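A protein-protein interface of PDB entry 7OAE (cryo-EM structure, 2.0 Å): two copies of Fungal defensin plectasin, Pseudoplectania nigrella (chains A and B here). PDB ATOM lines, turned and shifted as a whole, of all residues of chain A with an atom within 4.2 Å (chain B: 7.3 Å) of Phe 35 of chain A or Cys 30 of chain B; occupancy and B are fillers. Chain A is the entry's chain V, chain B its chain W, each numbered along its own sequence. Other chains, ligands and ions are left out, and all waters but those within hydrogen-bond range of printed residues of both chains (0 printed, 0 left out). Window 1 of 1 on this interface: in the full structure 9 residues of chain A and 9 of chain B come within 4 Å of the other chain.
The side-chain amide nitrogen (ND2) of Asn 5 of chain A lies within hydrogen-bond range of the backbone carbonyl oxygen (O) of Gly 6 of chain B (2.8 Å).
O of Gly 34 of chain A lies within hydrogen-bond range of N of Asn 5 of chain A (3.3 Å).
O of Leu 36 of chain A sits at hydrogen-bond distance from N of Ala 31 of chain A.
The side-chain sulfur (SG) of Cys 4 of chain B is disulfide-bonded to the side-chain sulfur (SG) of Cys 30 of chain B (2.0 Å).
O of Gly 6 of chain B is in hydrogen-bond range of OG of Ser 9 of chain B, at 3.0 Å.
The backbone carbonyl oxygen (O) of Gly 34 of chain B lies within hydrogen-bond range of the backbone NH (N) of Gly 6 of chain B, 2.8 Å away.
The side-chain sulfur (SG) of Cys 15 of chain B is disulfide-bonded to the side-chain sulfur (SG) of Cys 37 of chain B (2.0 Å).
Among the printed residues, pairs that only touch across the chains: Lys 32 of chain A with Tyr 29 of chain B (3.4 Å), Phe 35 of chain A with Tyr 29 of chain B (3.6 Å), Phe 35 of chain A with Cys 30 of chain B (3.5 Å), Phe 35 of chain A with Gly 33 of chain B (3.4 Å), Phe 35 of chain A with Gly 34 of chain B (3.5 Å) and Leu 36 of chain A with Tyr 29 of chain B (3.9 Å).
Of chain B, only Tyr 29 (3.6 Å), Cys 30 (3.5 Å), Gly 33 (3.4 Å) and Gly 34 (3.5 Å) come within 4 Å of Phe 35 of chain A.
No residue of chain B comes within 4 Å of Gly 34 of chain A.
Of the printed residues of chain A, Gly 34 of chain B touches Phe 35 (3.5 Å).
Of the printed residues of chain B, Leu 36 of chain A touches Tyr 29 (3.9 Å).
Printed residues of chain B within 4 Å of Asn 5 of chain A: Gly 6.
Printed residues of chain B within 4 Å of Lys 32 of chain A: Tyr 29.
Leu 36 of chain B touches none of the printed residues of chain A.
The nearest residue of chain B that does not touch Phe 35 of chain A is Ala 31 of chain B (5.3 Å).
The nearest printed residue of chain A that does not touch Cys 30 of chain B is Asn 5 of chain A (5.5 Å).
The nearest printed residue of chain A that does not touch Gly 33 of chain B is Asn 5 of chain A (5.6 Å).
Of the 11 printed residues of chain A, 4 touch a printed residue of chain B.
Hydrophobic or aromatic side chains of chain A within 4 Å of the printed part of chain B: Phe 35 and Leu 36.
Of the 21 printed residues of chain B, 5 touch a printed residue of chain A.
Printed residues of chain B that touch a printed residue of chain A: Gly 6, Tyr 29, Cys 30, Gly 33 and Gly 34.
Among the printed residues, no Asp or Glu carboxylate lies within 4 Å of a Lys or Arg side-chain nitrogen of the other chain.
Asn 5 of chain A touches Gly 6 of chain B, but with the chains exchanged Gly 6 of chain A does not touch Asn 5 of chain B (10.2 Å).
Phe 35 of chain A touches Gly 33 of chain B, but with the chains exchanged Gly 33 of chain A does not touch Phe 35 of chain B (10.8 Å).
Phe 35 of chain A touches Gly 34 of chain B, but with the chains exchanged Gly 34 of chain A does not touch Phe 35 of chain B (10.4 Å).
Positions printed for both chains: 1, 4, 5, 6, 31, 32, 33, 34, 35 and 36.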
ATOM      1  N   GLY A   1      -2.008  -2.933 -11.733  1.00  0.00           N
ATOM      2  CA  GLY A   1      -2.121  -1.802 -12.632  1.00  0.00           C
ATOM      3  C   GLY A   1      -2.449  -2.223 -14.044  1.00  0.00           C
ATOM      4  O   GLY A   1      -2.409  -3.407 -14.360  1.00  0.00           O
ATOM      5  N   CYS A   4      -5.015  -4.920 -14.307  1.00  0.00           N
ATOM      6  CA  CYS A   4      -4.806  -6.148 -13.548  1.00  0.00           C
ATOM      7  C   CYS A   4      -5.189  -5.864 -12.106  1.00  0.00           C
ATOM      8  O   CYS A   4      -4.402  -5.312 -11.341  1.00  0.00           O
ATOM      9  CB  CYS A   4      -3.364  -6.624 -13.667  1.00  0.00           C
ATOM     10  SG  CYS A   4      -2.957  -7.320 -15.264  1.00  0.00           S
ATOM     11  N   ASN A   5      -6.408  -6.227 -11.733  1.00  0.00           N
ATOM     12  CA  ASN A   5      -6.912  -5.910 -10.409  1.00  0.00           C
ATOM     13  C   ASN A   5      -7.688  -7.080  -9.832  1.00  0.00           C
ATOM     14  O   ASN A   5      -8.745  -6.901  -9.225  1.00  0.00           O
ATOM     15  CB  ASN A   5      -7.775  -4.655 -10.447  1.00  0.00           C
ATOM     16  CG  ASN A   5      -7.855  -3.970  -9.115  1.00  0.00           C
ATOM     17  OD1 ASN A   5      -7.072  -4.244  -8.217  1.00  0.00           O
ATOM     18  ND2 ASN A   5      -8.808  -3.071  -8.976  1.00  0.00           N
ATOM     19  N   GLY A   6      -7.178  -8.291 -10.004  1.00  0.00           N
ATOM     20  CA  GLY A   6      -7.789  -9.460  -9.425  1.00  0.00           C
ATOM     21  C   GLY A   6      -9.213  -9.670  -9.881  1.00  0.00           C
ATOM     22  O   GLY A   6      -9.515  -9.641 -11.071  1.00  0.00           O
ATOM     23  N   PRO A   7     -10.121  -9.892  -8.933  1.00  0.00           N
ATOM     24  CA  PRO A   7     -11.524 -10.098  -9.301  1.00  0.00           C
ATOM     25  C   PRO A   7     -12.164  -8.885  -9.929  1.00  0.00           C
ATOM     26  O   PRO A   7     -13.130  -9.034 -10.679  1.00  0.00           O
ATOM     27  CB  PRO A   7     -12.182 -10.437  -7.967  1.00  0.00           C
ATOM     28  CG  PRO A   7     -11.363  -9.743  -6.988  1.00  0.00           C
ATOM     29  CD  PRO A   7      -9.956  -9.803  -7.479  1.00  0.00           C
ATOM     30  N   ALA A  31       0.093 -11.302 -13.812  1.00  0.00           N
ATOM     31  CA  ALA A  31       0.884 -12.128 -12.918  1.00  0.00           C
ATOM     32  C   ALA A  31       0.631 -11.711 -11.474  1.00  0.00           C
ATOM     33  O   ALA A  31      -0.167 -10.817 -11.187  1.00  0.00           O
ATOM     34  CB  ALA A  31       2.358 -12.023 -13.277  1.00  0.00           C
ATOM     35  N   LYS A  32       1.346 -12.351 -10.553  1.00  0.00           N
ATOM     36  CA  LYS A  32       1.180 -12.143  -9.119  1.00  0.00           C
ATOM     37  C   LYS A  32      -0.255 -12.408  -8.690  1.00  0.00           C
ATOM     38  O   LYS A  32      -0.811 -11.715  -7.844  1.00  0.00           O
ATOM     39  CB  LYS A  32       1.623 -10.746  -8.705  1.00  0.00           C
ATOM     40  CG  LYS A  32       3.098 -10.501  -8.870  1.00  0.00           C
ATOM     41  CD  LYS A  32       3.875 -11.118  -7.738  1.00  0.00           C
ATOM     42  CE  LYS A  32       5.330 -10.710  -7.784  1.00  0.00           C
ATOM     43  NZ  LYS A  32       6.141 -11.641  -8.601  1.00  0.00           N
ATOM     44  N   GLY A  33      -0.854 -13.435  -9.274  1.00  0.00           N
ATOM     45  CA  GLY A  33      -2.205 -13.790  -8.912  1.00  0.00           C
ATOM     46  C   GLY A  33      -3.247 -12.818  -9.394  1.00  0.00           C
ATOM     47  O   GLY A  33      -4.287 -12.677  -8.759  1.00  0.00           O
ATOM     48  N   GLY A  34      -2.993 -12.138 -10.500  1.00  0.00           N
ATOM     49  CA  GLY A  34      -3.962 -11.247 -11.084  1.00  0.00           C
ATOM     50  C   GLY A  34      -3.772  -9.784 -10.786  1.00  0.00           C
ATOM     51  O   GLY A  34      -4.653  -8.990 -11.117  1.00  0.00           O
ATOM     52  N   PHE A  35      -2.654  -9.391 -10.193  1.00  0.00           N
ATOM     53  CA  PHE A  35      -2.492  -8.023  -9.739  1.00  0.00           C
ATOM     54  C   PHE A  35      -1.290  -7.295 -10.318  1.00  0.00           C
ATOM     55  O   PHE A  35      -1.035  -6.161  -9.912  1.00  0.00           O
ATOM     56  CB  PHE A  35      -2.413  -7.990  -8.212  1.00  0.00           C
ATOM     57  CG  PHE A  35      -3.698  -8.338  -7.546  1.00  0.00           C
ATOM     58  CD1 PHE A  35      -4.669  -7.384  -7.354  1.00  0.00           C
ATOM     59  CD2 PHE A  35      -3.946  -9.623  -7.128  1.00  0.00           C
ATOM     60  CE1 PHE A  35      -5.851  -7.705  -6.752  1.00  0.00           C
ATOM     61  CE2 PHE A  35      -5.127  -9.943  -6.526  1.00  0.00           C
ATOM     62  CZ  PHE A  35      -6.080  -8.984  -6.339  1.00  0.00           C
ATOM     63  N   LEU A  36      -0.552  -7.885 -11.248  1.00  0.00           N
ATOM     64  CA  LEU A  36       0.608  -7.221 -11.831  1.00  0.00           C
ATOM     65  C   LEU A  36       0.620  -7.447 -13.329  1.00  0.00           C
ATOM     66  O   LEU A  36       0.761  -8.580 -13.777  1.00  0.00           O
ATOM     67  CB  LEU A  36       1.900  -7.739 -11.208  1.00  0.00           C
ATOM     68  CG  LEU A  36       3.199  -7.330 -11.895  1.00  0.00           C
ATOM     69  CD1 LEU A  36       3.348  -5.834 -11.888  1.00  0.00           C
ATOM     70  CD2 LEU A  36       4.372  -7.973 -11.212  1.00  0.00           C
ATOM     71  N   GLY B   1      -2.323   1.700   1.062  1.00  0.00           N
ATOM     72  CA  GLY B   1      -1.765   3.007   0.771  1.00  0.00           C
ATOM     73  C   GLY B   1      -1.177   3.079  -0.618  1.00  0.00           C
ATOM     74  O   GLY B   1      -1.128   2.076  -1.323  1.00  0.00           O
ATOM     75  N   PHE B   2      -0.737   4.273  -1.006  1.00  0.00           N
ATOM     76  CA  PHE B   2      -0.135   4.511  -2.312  1.00  0.00           C
ATOM     77  C   PHE B   2      -1.061   4.110  -3.449  1.00  0.00           C
ATOM     78  O   PHE B   2      -0.612   3.624  -4.484  1.00  0.00           O
ATOM     79  CB  PHE B   2       1.204   3.789  -2.442  1.00  0.00           C
ATOM     80  CG  PHE B   2       2.228   4.248  -1.464  1.00  0.00           C
ATOM     81  CD1 PHE B   2       2.796   5.499  -1.581  1.00  0.00           C
ATOM     82  CD2 PHE B   2       2.620   3.437  -0.424  1.00  0.00           C
ATOM     83  CE1 PHE B   2       3.736   5.927  -0.684  1.00  0.00           C
ATOM     84  CE2 PHE B   2       3.562   3.861   0.477  1.00  0.00           C
ATOM     85  CZ  PHE B   2       4.121   5.107   0.345  1.00  0.00           C
ATOM     86  N   GLY B   3      -2.359   4.304  -3.270  1.00  0.00           N
ATOM     87  CA  GLY B   3      -3.310   4.057  -4.324  1.00  0.00           C
ATOM     88  C   GLY B   3      -3.745   2.620  -4.487  1.00  0.00           C
ATOM     89  O   GLY B   3      -4.489   2.323  -5.424  1.00  0.00           O
ATOM     90  N   CYS B   4      -3.302   1.717  -3.622  1.00  0.00           N
ATOM     91  CA  CYS B   4      -3.764   0.334  -3.661  1.00  0.00           C
ATOM     92  C   CYS B   4      -5.030   0.246  -2.827  1.00  0.00           C
ATOM     93  O   CYS B   4      -4.977   0.197  -1.601  1.00  0.00           O
ATOM     94  CB  CYS B   4      -2.686  -0.609  -3.149  1.00  0.00           C
ATOM     95  SG  CYS B   4      -1.335  -0.859  -4.303  1.00  0.00           S
ATOM     96  N   ASN B   5      -6.179   0.237  -3.489  1.00  0.00           N
ATOM     97  CA  ASN B   5      -7.448   0.327  -2.788  1.00  0.00           C
ATOM     98  C   ASN B   5      -8.466  -0.628  -3.380  1.00  0.00           C
ATOM     99  O   ASN B   5      -9.637  -0.284  -3.544  1.00  0.00           O
ATOM    100  CB  ASN B   5      -7.976   1.756  -2.811  1.00  0.00           C
ATOM    101  CG  ASN B   5      -8.898   2.047  -1.663  1.00  0.00           C
ATOM    102  OD1 ASN B   5      -8.938   1.310  -0.686  1.00  0.00           O
ATOM    103  ND2 ASN B   5      -9.652   3.125  -1.772  1.00  0.00           N
ATOM    104  N   GLY B   6      -8.042  -1.841  -3.705  1.00  0.00           N
ATOM    105  CA  GLY B   6      -8.941  -2.860  -4.181  1.00  0.00           C
ATOM    106  C   GLY B   6      -9.706  -2.448  -5.416  1.00  0.00           C
ATOM    107  O   GLY B   6      -9.134  -1.994  -6.403  1.00  0.00           O
ATOM    108  N   SER B   9      -9.186   1.198  -6.779  1.00  0.00           N
ATOM    109  CA  SER B   9      -7.871   1.646  -7.197  1.00  0.00           C
ATOM    110  C   SER B   9      -7.950   2.376  -8.527  1.00  0.00           C
ATOM    111  O   SER B   9      -8.819   2.115  -9.358  1.00  0.00           O
ATOM    112  CB  SER B   9      -6.916   0.464  -7.319  1.00  0.00           C
ATOM    113  OG  SER B   9      -6.753  -0.192  -6.081  1.00  0.00           O
ATOM    114  N   GLU B  10      -7.026   3.304  -8.719  1.00  0.00           N
ATOM    115  CA  GLU B  10      -6.850   4.002  -9.979  1.00  0.00           C
ATOM    116  C   GLU B  10      -5.439   3.748 -10.485  1.00  0.00           C
ATOM    117  O   GLU B  10      -4.512   3.545  -9.697  1.00  0.00           O
ATOM    118  CB  GLU B  10      -7.076   5.497  -9.811  1.00  0.00           C
ATOM    119  CG  GLU B  10      -8.364   5.833  -9.105  1.00  0.00           C
ATOM    120  CD  GLU B  10      -8.377   7.245  -8.569  1.00  0.00           C
ATOM    121  OE1 GLU B  10      -7.871   8.151  -9.259  1.00  0.00           O
ATOM    122  OE2 GLU B  10      -8.879   7.449  -7.446  1.00  0.00           O
ATOM    123  N   ASP B  12      -2.848   5.236 -11.045  1.00  0.00           N
ATOM    124  CA  ASP B  12      -2.225   6.513 -10.734  1.00  0.00           C
ATOM    125  C   ASP B  12      -0.710   6.435 -10.592  1.00  0.00           C
ATOM    126  O   ASP B  12      -0.072   7.474 -10.402  1.00  0.00           O
ATOM    127  CB  ASP B  12      -2.833   7.084  -9.452  1.00  0.00           C
ATOM    128  CG  ASP B  12      -2.892   6.066  -8.331  1.00  0.00           C
ATOM    129  OD1 ASP B  12      -2.230   5.013  -8.440  1.00  0.00           O
ATOM    130  OD2 ASP B  12      -3.612   6.314  -7.342  1.00  0.00           O
ATOM    131  N   CYS B  15       1.984   3.669  -6.424  1.00  0.00           N
ATOM    132  CA  CYS B  15       2.751   2.527  -5.945  1.00  0.00           C
ATOM    133  C   CYS B  15       4.029   2.360  -6.751  1.00  0.00           C
ATOM    134  O   CYS B  15       5.100   2.109  -6.189  1.00  0.00           O
ATOM    135  CB  CYS B  15       1.898   1.262  -6.010  1.00  0.00           C
ATOM    136  SG  CYS B  15       2.619  -0.216  -5.268  1.00  0.00           S
ATOM    137  N   GLY B  28       6.113  -1.708  -8.666  1.00  0.00           N
ATOM    138  CA  GLY B  28       5.291  -2.143  -7.557  1.00  0.00           C
ATOM    139  C   GLY B  28       3.937  -2.594  -8.049  1.00  0.00           C
ATOM    140  O   GLY B  28       3.511  -2.261  -9.155  1.00  0.00           O
ATOM    141  N   TYR B  29       3.266  -3.365  -7.208  1.00  0.00           N
ATOM    142  CA  TYR B  29       1.926  -3.836  -7.509  1.00  0.00           C
ATOM    143  C   TYR B  29       1.145  -3.908  -6.210  1.00  0.00           C
ATOM    144  O   TYR B  29       1.704  -3.793  -5.123  1.00  0.00           O
ATOM    145  CB  TYR B  29       1.954  -5.191  -8.219  1.00  0.00           C
ATOM    146  CG  TYR B  29       2.333  -6.326  -7.319  1.00  0.00           C
ATOM    147  CD1 TYR B  29       3.651  -6.551  -6.981  1.00  0.00           C
ATOM    148  CD2 TYR B  29       1.374  -7.167  -6.797  1.00  0.00           C
ATOM    149  CE1 TYR B  29       3.999  -7.576  -6.154  1.00  0.00           C
ATOM    150  CE2 TYR B  29       1.715  -8.195  -5.970  1.00  0.00           C
ATOM    151  CZ  TYR B  29       3.029  -8.397  -5.651  1.00  0.00           C
ATOM    152  OH  TYR B  29       3.371  -9.429  -4.820  1.00  0.00           O
ATOM    153  N   CYS B  30      -0.156  -4.104  -6.323  1.00  0.00           N
ATOM    154  CA  CYS B  30      -1.034  -4.121  -5.159  1.00  0.00           C
ATOM    155  C   CYS B  30      -1.209  -5.562  -4.696  1.00  0.00           C
ATOM    156  O   CYS B  30      -2.044  -6.297  -5.219  1.00  0.00           O
ATOM    157  CB  CYS B  30      -2.365  -3.459  -5.488  1.00  0.00           C
ATOM    158  SG  CYS B  30      -2.221  -1.714  -5.917  1.00  0.00           S
ATOM    159  N   ALA B  31      -0.414  -5.960  -3.715  1.00  0.00           N
ATOM    160  CA  ALA B  31      -0.514  -7.266  -3.086  1.00  0.00           C
ATOM    161  C   ALA B  31      -1.590  -7.235  -2.008  1.00  0.00           C
ATOM    162  O   ALA B  31      -2.291  -6.238  -1.822  1.00  0.00           O
ATOM    163  CB  ALA B  31       0.834  -7.676  -2.513  1.00  0.00           C
ATOM    164  N   LYS B  32      -1.701  -8.330  -1.260  1.00  0.00           N
ATOM    165  CA  LYS B  32      -2.765  -8.526  -0.281  1.00  0.00           C
ATOM    166  C   LYS B  32      -4.131  -8.360  -0.925  1.00  0.00           C
ATOM    167  O   LYS B  32      -5.042  -7.767  -0.356  1.00  0.00           O
ATOM    168  CB  LYS B  32      -2.612  -7.583   0.906  1.00  0.00           C
ATOM    169  CG  LYS B  32      -1.413  -7.861   1.760  1.00  0.00           C
ATOM    170  CD  LYS B  32      -1.582  -9.144   2.522  1.00  0.00           C
ATOM    171  CE  LYS B  32      -0.457  -9.333   3.509  1.00  0.00           C
ATOM    172  NZ  LYS B  32      -0.557 -10.650   4.184  1.00  0.00           N
ATOM    173  N   GLY B  33      -4.273  -8.889  -2.129  1.00  0.00           N
ATOM    174  CA  GLY B  33      -5.542  -8.811  -2.811  1.00  0.00           C
ATOM    175  C   GLY B  33      -5.908  -7.427  -3.274  1.00  0.00           C
ATOM    176  O   GLY B  33      -7.089  -7.118  -3.392  1.00  0.00           O
ATOM    177  N   GLY B  34      -4.923  -6.582  -3.536  1.00  0.00           N
ATOM    178  CA  GLY B  34      -5.169  -5.260  -4.049  1.00  0.00           C
ATOM    179  C   GLY B  34      -5.130  -4.142  -3.041  1.00  0.00           C
ATOM    180  O   GLY B  34      -5.552  -3.034  -3.368  1.00  0.00           O
ATOM    181  N   PHE B  35      -4.628  -4.380  -1.837  1.00  0.00           N
ATOM    182  CA  PHE B  35      -4.694  -3.381  -0.788  1.00  0.00           C
ATOM    183  C   PHE B  35      -3.357  -3.024  -0.162  1.00  0.00           C
ATOM    184  O   PHE B  35      -3.343  -2.261   0.804  1.00  0.00           O
ATOM    185  CB  PHE B  35      -5.655  -3.839   0.310  1.00  0.00           C
ATOM    186  CG  PHE B  35      -7.080  -3.881  -0.124  1.00  0.00           C
ATOM    187  CD1 PHE B  35      -7.857  -2.747  -0.091  1.00  0.00           C
ATOM    188  CD2 PHE B  35      -7.642  -5.049  -0.576  1.00  0.00           C
ATOM    189  CE1 PHE B  35      -9.158  -2.785  -0.496  1.00  0.00           C
ATOM    190  CE2 PHE B  35      -8.942  -5.086  -0.981  1.00  0.00           C
ATOM    191  CZ  PHE B  35      -9.701  -3.954  -0.940  1.00  0.00           C
ATOM    192  N   LEU B  36      -2.236  -3.529  -0.667  1.00  0.00           N
ATOM    193  CA  LEU B  36      -0.936  -3.214  -0.087  1.00  0.00           C
ATOM    194  C   LEU B  36       0.082  -2.995  -1.192  1.00  0.00           C
ATOM    195  O   LEU B  36       0.342  -3.903  -1.975  1.00  0.00           O
ATOM    196  CB  LEU B  36      -0.471  -4.333   0.840  1.00  0.00           C
ATOM    197  CG  LEU B  36       0.970  -4.232   1.324  1.00  0.00           C
ATOM    198  CD1 LEU B  36       1.147  -2.999   2.165  1.00  0.00           C
ATOM    199  CD2 LEU B  36       1.347  -5.456   2.107  1.00  0.00           C
ATOM    200  N   CYS B  37       0.675  -1.810  -1.245  1.00  0.00           N
ATOM    201  CA  CYS B  37       1.714  -1.558  -2.234  1.00  0.00           C
ATOM    202  C   CYS B  37       2.941  -2.398  -1.912  1.00  0.00           C
ATOM    203  O   CYS B  37       3.501  -2.302  -0.818  1.00  0.00           O
ATOM    204  CB  CYS B  37       2.072  -0.077  -2.270  1.00  0.00           C
ATOM    205  SG  CYS B  37       3.344   0.375  -3.465  1.00  0.00           S
ATOM    206  N   LYS B  38       3.359  -3.221  -2.863  1.00  0.00           N
ATOM    207  CA  LYS B  38       4.462  -4.149  -2.690  1.00  0.00           C
ATOM    208  C   LYS B  38       5.451  -3.938  -3.818  1.00  0.00           C
ATOM    209  O   LYS B  38       5.063  -3.918  -4.988  1.00  0.00           O
ATOM    210  CB  LYS B  38       3.960  -5.591  -2.686  1.00  0.00           C
ATOM    211  CG  LYS B  38       5.043  -6.632  -2.610  1.00  0.00           C
ATOM    212  CD  LYS B  38       5.540  -6.801  -1.203  1.00  0.00           C
ATOM    213  CE  LYS B  38       6.642  -7.835  -1.152  1.00  0.00           C
ATOM    214  NZ  LYS B  38       6.977  -8.200   0.245  1.00  0.00           N
